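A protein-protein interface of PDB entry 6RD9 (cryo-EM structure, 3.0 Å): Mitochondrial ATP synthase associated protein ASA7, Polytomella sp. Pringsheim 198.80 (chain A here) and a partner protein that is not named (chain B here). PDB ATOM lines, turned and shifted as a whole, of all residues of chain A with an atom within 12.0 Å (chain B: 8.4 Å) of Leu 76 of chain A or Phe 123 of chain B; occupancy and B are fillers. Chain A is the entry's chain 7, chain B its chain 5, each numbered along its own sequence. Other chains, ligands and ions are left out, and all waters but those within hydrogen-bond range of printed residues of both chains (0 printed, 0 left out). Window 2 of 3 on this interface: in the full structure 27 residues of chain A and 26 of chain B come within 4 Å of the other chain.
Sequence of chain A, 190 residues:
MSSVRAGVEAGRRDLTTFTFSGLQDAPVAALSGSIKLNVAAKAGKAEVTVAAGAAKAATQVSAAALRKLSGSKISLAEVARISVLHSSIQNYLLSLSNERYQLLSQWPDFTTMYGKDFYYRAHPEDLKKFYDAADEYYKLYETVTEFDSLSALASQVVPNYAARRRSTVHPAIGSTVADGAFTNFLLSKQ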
ATOM      1  N   LEU A  15     -21.901   2.195 -26.904  1.00  0.00           N
ATOM      2  CA  LEU A  15     -21.165   1.202 -27.657  1.00  0.00           C
ATOM      3  C   LEU A  15     -22.101   0.354 -28.481  1.00  0.00           C
ATOM      4  O   LEU A  15     -23.270   0.212 -28.149  1.00  0.00           O
ATOM      5  CB  LEU A  15     -20.345   0.326 -26.727  1.00  0.00           C
ATOM      6  CG  LEU A  15     -18.859   0.619 -26.716  1.00  0.00           C
ATOM      7  CD1 LEU A  15     -18.194  -0.348 -25.809  1.00  0.00           C
ATOM      8  CD2 LEU A  15     -18.319   0.460 -28.108  1.00  0.00           C
ATOM      9  N   SER A  72     -20.998  -7.919 -22.610  1.00  0.00           N
ATOM     10  CA  SER A  72     -21.899  -7.261 -21.679  1.00  0.00           C
ATOM     11  C   SER A  72     -21.262  -5.943 -21.269  1.00  0.00           C
ATOM     12  O   SER A  72     -20.191  -5.935 -20.666  1.00  0.00           O
ATOM     13  CB  SER A  72     -22.166  -8.140 -20.464  1.00  0.00           C
ATOM     14  OG  SER A  72     -20.957  -8.653 -19.951  1.00  0.00           O
ATOM     15  N   LYS A  73     -21.918  -4.840 -21.598  1.00  0.00           N
ATOM     16  CA  LYS A  73     -21.311  -3.534 -21.440  1.00  0.00           C
ATOM     17  C   LYS A  73     -21.380  -3.068 -19.995  1.00  0.00           C
ATOM     18  O   LYS A  73     -22.226  -3.515 -19.219  1.00  0.00           O
ATOM     19  CB  LYS A  73     -22.003  -2.521 -22.340  1.00  0.00           C
ATOM     20  CG  LYS A  73     -22.076  -2.930 -23.786  1.00  0.00           C
ATOM     21  CD  LYS A  73     -20.798  -2.636 -24.494  1.00  0.00           C
ATOM     22  CE  LYS A  73     -20.730  -3.371 -25.809  1.00  0.00           C
ATOM     23  NZ  LYS A  73     -22.053  -3.456 -26.442  1.00  0.00           N
ATOM     24  N   ILE A  74     -20.478  -2.161 -19.632  1.00  0.00           N
ATOM     25  CA  ILE A  74     -20.494  -1.614 -18.279  1.00  0.00           C
ATOM     26  C   ILE A  74     -21.590  -0.571 -18.140  1.00  0.00           C
ATOM     27  O   ILE A  74     -22.454  -0.681 -17.263  1.00  0.00           O
ATOM     28  CB  ILE A  74     -19.125  -1.032 -17.899  1.00  0.00           C
ATOM     29  CG1 ILE A  74     -18.097  -2.140 -17.755  1.00  0.00           C
ATOM     30  CG2 ILE A  74     -19.228  -0.321 -16.583  1.00  0.00           C
ATOM     31  CD1 ILE A  74     -18.368  -3.048 -16.601  1.00  0.00           C
ATOM     32  N   SER A  75     -21.560   0.448 -19.004  1.00  0.00           N
ATOM     33  CA  SER A  75     -22.534   1.539 -19.069  1.00  0.00           C
ATOM     34  C   SER A  75     -22.597   2.309 -17.749  1.00  0.00           C
ATOM     35  O   SER A  75     -23.542   2.212 -16.970  1.00  0.00           O
ATOM     36  CB  SER A  75     -23.914   1.047 -19.501  1.00  0.00           C
ATOM     37  OG  SER A  75     -24.784   2.147 -19.652  1.00  0.00           O
ATOM     38  N   LEU A  76     -21.511   3.034 -17.513  1.00  0.00           N
ATOM     39  CA  LEU A  76     -21.367   3.866 -16.334  1.00  0.00           C
ATOM     40  C   LEU A  76     -22.371   5.000 -16.346  1.00  0.00           C
ATOM     41  O   LEU A  76     -22.758   5.506 -17.397  1.00  0.00           O
ATOM     42  CB  LEU A  76     -19.966   4.439 -16.280  1.00  0.00           C
ATOM     43  CG  LEU A  76     -18.891   3.401 -16.120  1.00  0.00           C
ATOM     44  CD1 LEU A  76     -17.621   4.089 -16.309  1.00  0.00           C
ATOM     45  CD2 LEU A  76     -18.995   2.872 -14.746  1.00  0.00           C
ATOM     46  N   ALA A  77     -22.794   5.401 -15.156  1.00  0.00           N
ATOM     47  CA  ALA A  77     -23.750   6.480 -15.044  1.00  0.00           C
ATOM     48  C   ALA A  77     -23.544   7.172 -13.721  1.00  0.00           C
ATOM     49  O   ALA A  77     -23.180   6.546 -12.729  1.00  0.00           O
ATOM     50  CB  ALA A  77     -25.181   5.987 -15.149  1.00  0.00           C
ATOM     51  N   GLU A  78     -23.806   8.465 -13.715  1.00  0.00           N
ATOM     52  CA  GLU A  78     -23.395   9.327 -12.632  1.00  0.00           C
ATOM     53  C   GLU A  78     -24.445   9.332 -11.543  1.00  0.00           C
ATOM     54  O   GLU A  78     -25.634   9.491 -11.819  1.00  0.00           O
ATOM     55  CB  GLU A  78     -23.160  10.733 -13.156  1.00  0.00           C
ATOM     56  CG  GLU A  78     -22.229  10.728 -14.320  1.00  0.00           C
ATOM     57  CD  GLU A  78     -21.777  12.092 -14.706  1.00  0.00           C
ATOM     58  OE1 GLU A  78     -22.223  13.053 -14.071  1.00  0.00           O
ATOM     59  OE2 GLU A  78     -20.974  12.218 -15.644  1.00  0.00           O
ATOM     60  N   VAL A  79     -24.001   9.151 -10.310  1.00  0.00           N
ATOM     61  CA  VAL A  79     -24.865   9.258  -9.149  1.00  0.00           C
ATOM     62  C   VAL A  79     -24.749  10.685  -8.647  1.00  0.00           C
ATOM     63  O   VAL A  79     -23.726  11.073  -8.088  1.00  0.00           O
ATOM     64  CB  VAL A  79     -24.472   8.254  -8.069  1.00  0.00           C
ATOM     65  CG1 VAL A  79     -25.287   8.486  -6.844  1.00  0.00           C
ATOM     66  CG2 VAL A  79     -24.683   6.878  -8.582  1.00  0.00           C
ATOM     67  N   ALA A  80     -25.785  11.473  -8.858  1.00  0.00           N
ATOM     68  CA  ALA A  80     -25.756  12.878  -8.523  1.00  0.00           C
ATOM     69  C   ALA A  80     -26.643  13.131  -7.324  1.00  0.00           C
ATOM     70  O   ALA A  80     -27.526  12.339  -7.009  1.00  0.00           O
ATOM     71  CB  ALA A  80     -26.208  13.719  -9.703  1.00  0.00           C
ATOM     72  N   ARG A  81     -26.375  14.232  -6.632  1.00  0.00           N
ATOM     73  CA  ARG A  81     -27.183  14.561  -5.471  1.00  0.00           C
ATOM     74  C   ARG A  81     -28.576  14.957  -5.894  1.00  0.00           C
ATOM     75  O   ARG A  81     -29.563  14.464  -5.349  1.00  0.00           O
ATOM     76  CB  ARG A  81     -26.546  15.680  -4.669  1.00  0.00           C
ATOM     77  CG  ARG A  81     -27.418  16.143  -3.559  1.00  0.00           C
ATOM     78  CD  ARG A  81     -26.662  16.927  -2.571  1.00  0.00           C
ATOM     79  NE  ARG A  81     -27.533  17.454  -1.539  1.00  0.00           N
ATOM     80  CZ  ARG A  81     -28.003  18.688  -1.543  1.00  0.00           C
ATOM     81  NH1 ARG A  81     -28.782  19.108  -0.569  1.00  0.00           N
ATOM     82  NH2 ARG A  81     -27.689  19.500  -2.531  1.00  0.00           N
ATOM     83  N   VAL A  84     -27.509  15.590 -12.886  1.00  0.00           N
ATOM     84  CA  VAL A  84     -26.248  15.888 -13.541  1.00  0.00           C
ATOM     85  C   VAL A  84     -26.247  17.302 -14.074  1.00  0.00           C
ATOM     86  O   VAL A  84     -25.199  17.944 -14.137  1.00  0.00           O
ATOM     87  CB  VAL A  84     -25.996  14.858 -14.643  1.00  0.00           C
ATOM     88  CG1 VAL A  84     -24.643  14.987 -15.181  1.00  0.00           C
ATOM     89  CG2 VAL A  84     -26.128  13.511 -14.073  1.00  0.00           C
ATOM     90  N   TRP B 116     -19.229  15.429  -3.957  1.00  0.00           N
ATOM     91  CA  TRP B 116     -20.200  14.547  -4.568  1.00  0.00           C
ATOM     92  C   TRP B 116     -21.406  15.308  -5.042  1.00  0.00           C
ATOM     93  O   TRP B 116     -22.277  14.730  -5.687  1.00  0.00           O
ATOM     94  CB  TRP B 116     -20.616  13.461  -3.586  1.00  0.00           C
ATOM     95  CG  TRP B 116     -19.464  12.885  -2.892  1.00  0.00           C
ATOM     96  CD1 TRP B 116     -19.139  13.054  -1.601  1.00  0.00           C
ATOM     97  CD2 TRP B 116     -18.453  12.062  -3.459  1.00  0.00           C
ATOM     98  NE1 TRP B 116     -17.991  12.388  -1.312  1.00  0.00           N
ATOM     99  CE2 TRP B 116     -17.545  11.772  -2.446  1.00  0.00           C
ATOM    100  CE3 TRP B 116     -18.228  11.543  -4.731  1.00  0.00           C
ATOM    101  CZ2 TRP B 116     -16.441  10.983  -2.654  1.00  0.00           C
ATOM    102  CZ3 TRP B 116     -17.128  10.770  -4.935  1.00  0.00           C
ATOM    103  CH2 TRP B 116     -16.248  10.494  -3.908  1.00  0.00           C
ATOM    104  N   PRO B 120     -20.392  14.635  -9.704  1.00  0.00           N
ATOM    105  CA  PRO B 120     -21.041  13.387  -9.320  1.00  0.00           C
ATOM    106  C   PRO B 120     -20.260  12.177  -9.794  1.00  0.00           C
ATOM    107  O   PRO B 120     -19.686  12.168 -10.882  1.00  0.00           O
ATOM    108  CB  PRO B 120     -22.402  13.481 -10.005  1.00  0.00           C
ATOM    109  CG  PRO B 120     -22.226  14.417 -11.064  1.00  0.00           C
ATOM    110  CD  PRO B 120     -21.235  15.407 -10.619  1.00  0.00           C
ATOM    111  N   ALA B 121     -20.236  11.161  -8.947  1.00  0.00           N
ATOM    112  CA  ALA B 121     -19.360  10.020  -9.128  1.00  0.00           C
ATOM    113  C   ALA B 121     -19.875   9.105 -10.218  1.00  0.00           C
ATOM    114  O   ALA B 121     -21.073   8.850 -10.309  1.00  0.00           O
ATOM    115  CB  ALA B 121     -19.252   9.248  -7.823  1.00  0.00           C
ATOM    116  N   LEU B 122     -18.965   8.592 -11.025  1.00  0.00           N
ATOM    117  CA  LEU B 122     -19.303   7.598 -12.026  1.00  0.00           C
ATOM    118  C   LEU B 122     -19.337   6.226 -11.384  1.00  0.00           C
ATOM    119  O   LEU B 122     -18.302   5.706 -10.975  1.00  0.00           O
ATOM    120  CB  LEU B 122     -18.284   7.621 -13.149  1.00  0.00           C
ATOM    121  CG  LEU B 122     -18.601   8.601 -14.239  1.00  0.00           C
ATOM    122  CD1 LEU B 122     -17.469   8.680 -15.187  1.00  0.00           C
ATOM    123  CD2 LEU B 122     -19.773   8.072 -14.923  1.00  0.00           C
ATOM    124  N   PHE B 123     -20.508   5.629 -11.310  1.00  0.00           N
ATOM    125  CA  PHE B 123     -20.606   4.309 -10.730  1.00  0.00           C
ATOM    126  C   PHE B 123     -20.854   3.233 -11.769  1.00  0.00           C
ATOM    127  O   PHE B 123     -21.627   3.423 -12.701  1.00  0.00           O
ATOM    128  CB  PHE B 123     -21.704   4.287  -9.687  1.00  0.00           C
ATOM    129  CG  PHE B 123     -21.233   4.635  -8.334  1.00  0.00           C
ATOM    130  CD1 PHE B 123     -20.734   3.666  -7.506  1.00  0.00           C
ATOM    131  CD2 PHE B 123     -21.270   5.927  -7.888  1.00  0.00           C
ATOM    132  CE1 PHE B 123     -20.295   3.984  -6.251  1.00  0.00           C
ATOM    133  CE2 PHE B 123     -20.830   6.249  -6.635  1.00  0.00           C
ATOM    134  CZ  PHE B 123     -20.341   5.276  -5.820  1.00  0.00           C
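The backbone carbonyl oxygen of Ala 121 of chain B sits at hydrogen-bond distance from the backbone NH of Val 79 of chain A, 2.9 Å away. The backbone NH of Phe 123 of chain B sits at hydrogen-bond distance from the backbone carbonyl oxygen of Ala 77 of chain A, 3.2 Å away.
CD2 of Leu 122 of chain B touches CB of Leu 76 of chain A, 3.9 Å away. CD2 of Leu 76 of chain A touches O of Phe 123 of chain B (3.4 Å). Ala 121 of chain B touches Ala 77 of chain A. OE1 of Glu 78 of chain A touches CG of Pro 120 of chain B, at 3.3 Å. CA of Glu 78 of chain A touches O of Ala 121 of chain B (3.3 Å). Glu 78 of chain A touches Leu 122 of chain B. Val 79 of chain A touches Pro 120 of chain B. Val 79 of chain A touches Phe 123 of chain B. Ala 80 of chain A touches Pro 120 of chain B.
Of chain B, only Leu 122 (3.9 Å) and Phe 123 (3.4 Å) come within 4 Å of Leu 76 of chain A. Phe 123 of chain B touches just these residues of chain A: Leu 76 (3.4 Å), Ala 77 (3.2 Å) and Val 79 (3.6 Å). No residue of chain B comes within 4 Å of Ser 75 of chain A. Of chain A, only Ala 77, Glu 78 and Val 79 come within 4 Å of Ala 121 of chain B. Of the printed residues of chain B, Glu 78 of chain A touches Pro 120, Ala 121 and Leu 122. Of the printed residues of chain B, Ala 80 of chain A touches Pro 120 (3.7 Å). Printed residues of chain B within 4 Å of Val 79 of chain A: Pro 120, Ala 121 and Phe 123. Printed residues of chain A within 4 Å of Pro 120 of chain B: Glu 78 (3.3 Å), Val 79 (3.4 Å) and Ala 80 (3.7 Å). Lys 73 of chain A touches none of the printed residues of chain B. The nearest residue of chain A that does not touch Phe 123 of chain B is Ser 75 of chain A (4.8 Å).
Along chain A the printed residues that touch a printed residue of chain B span positions 76 to 80. Among the printed residues, 11 pairs touch across the chains.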
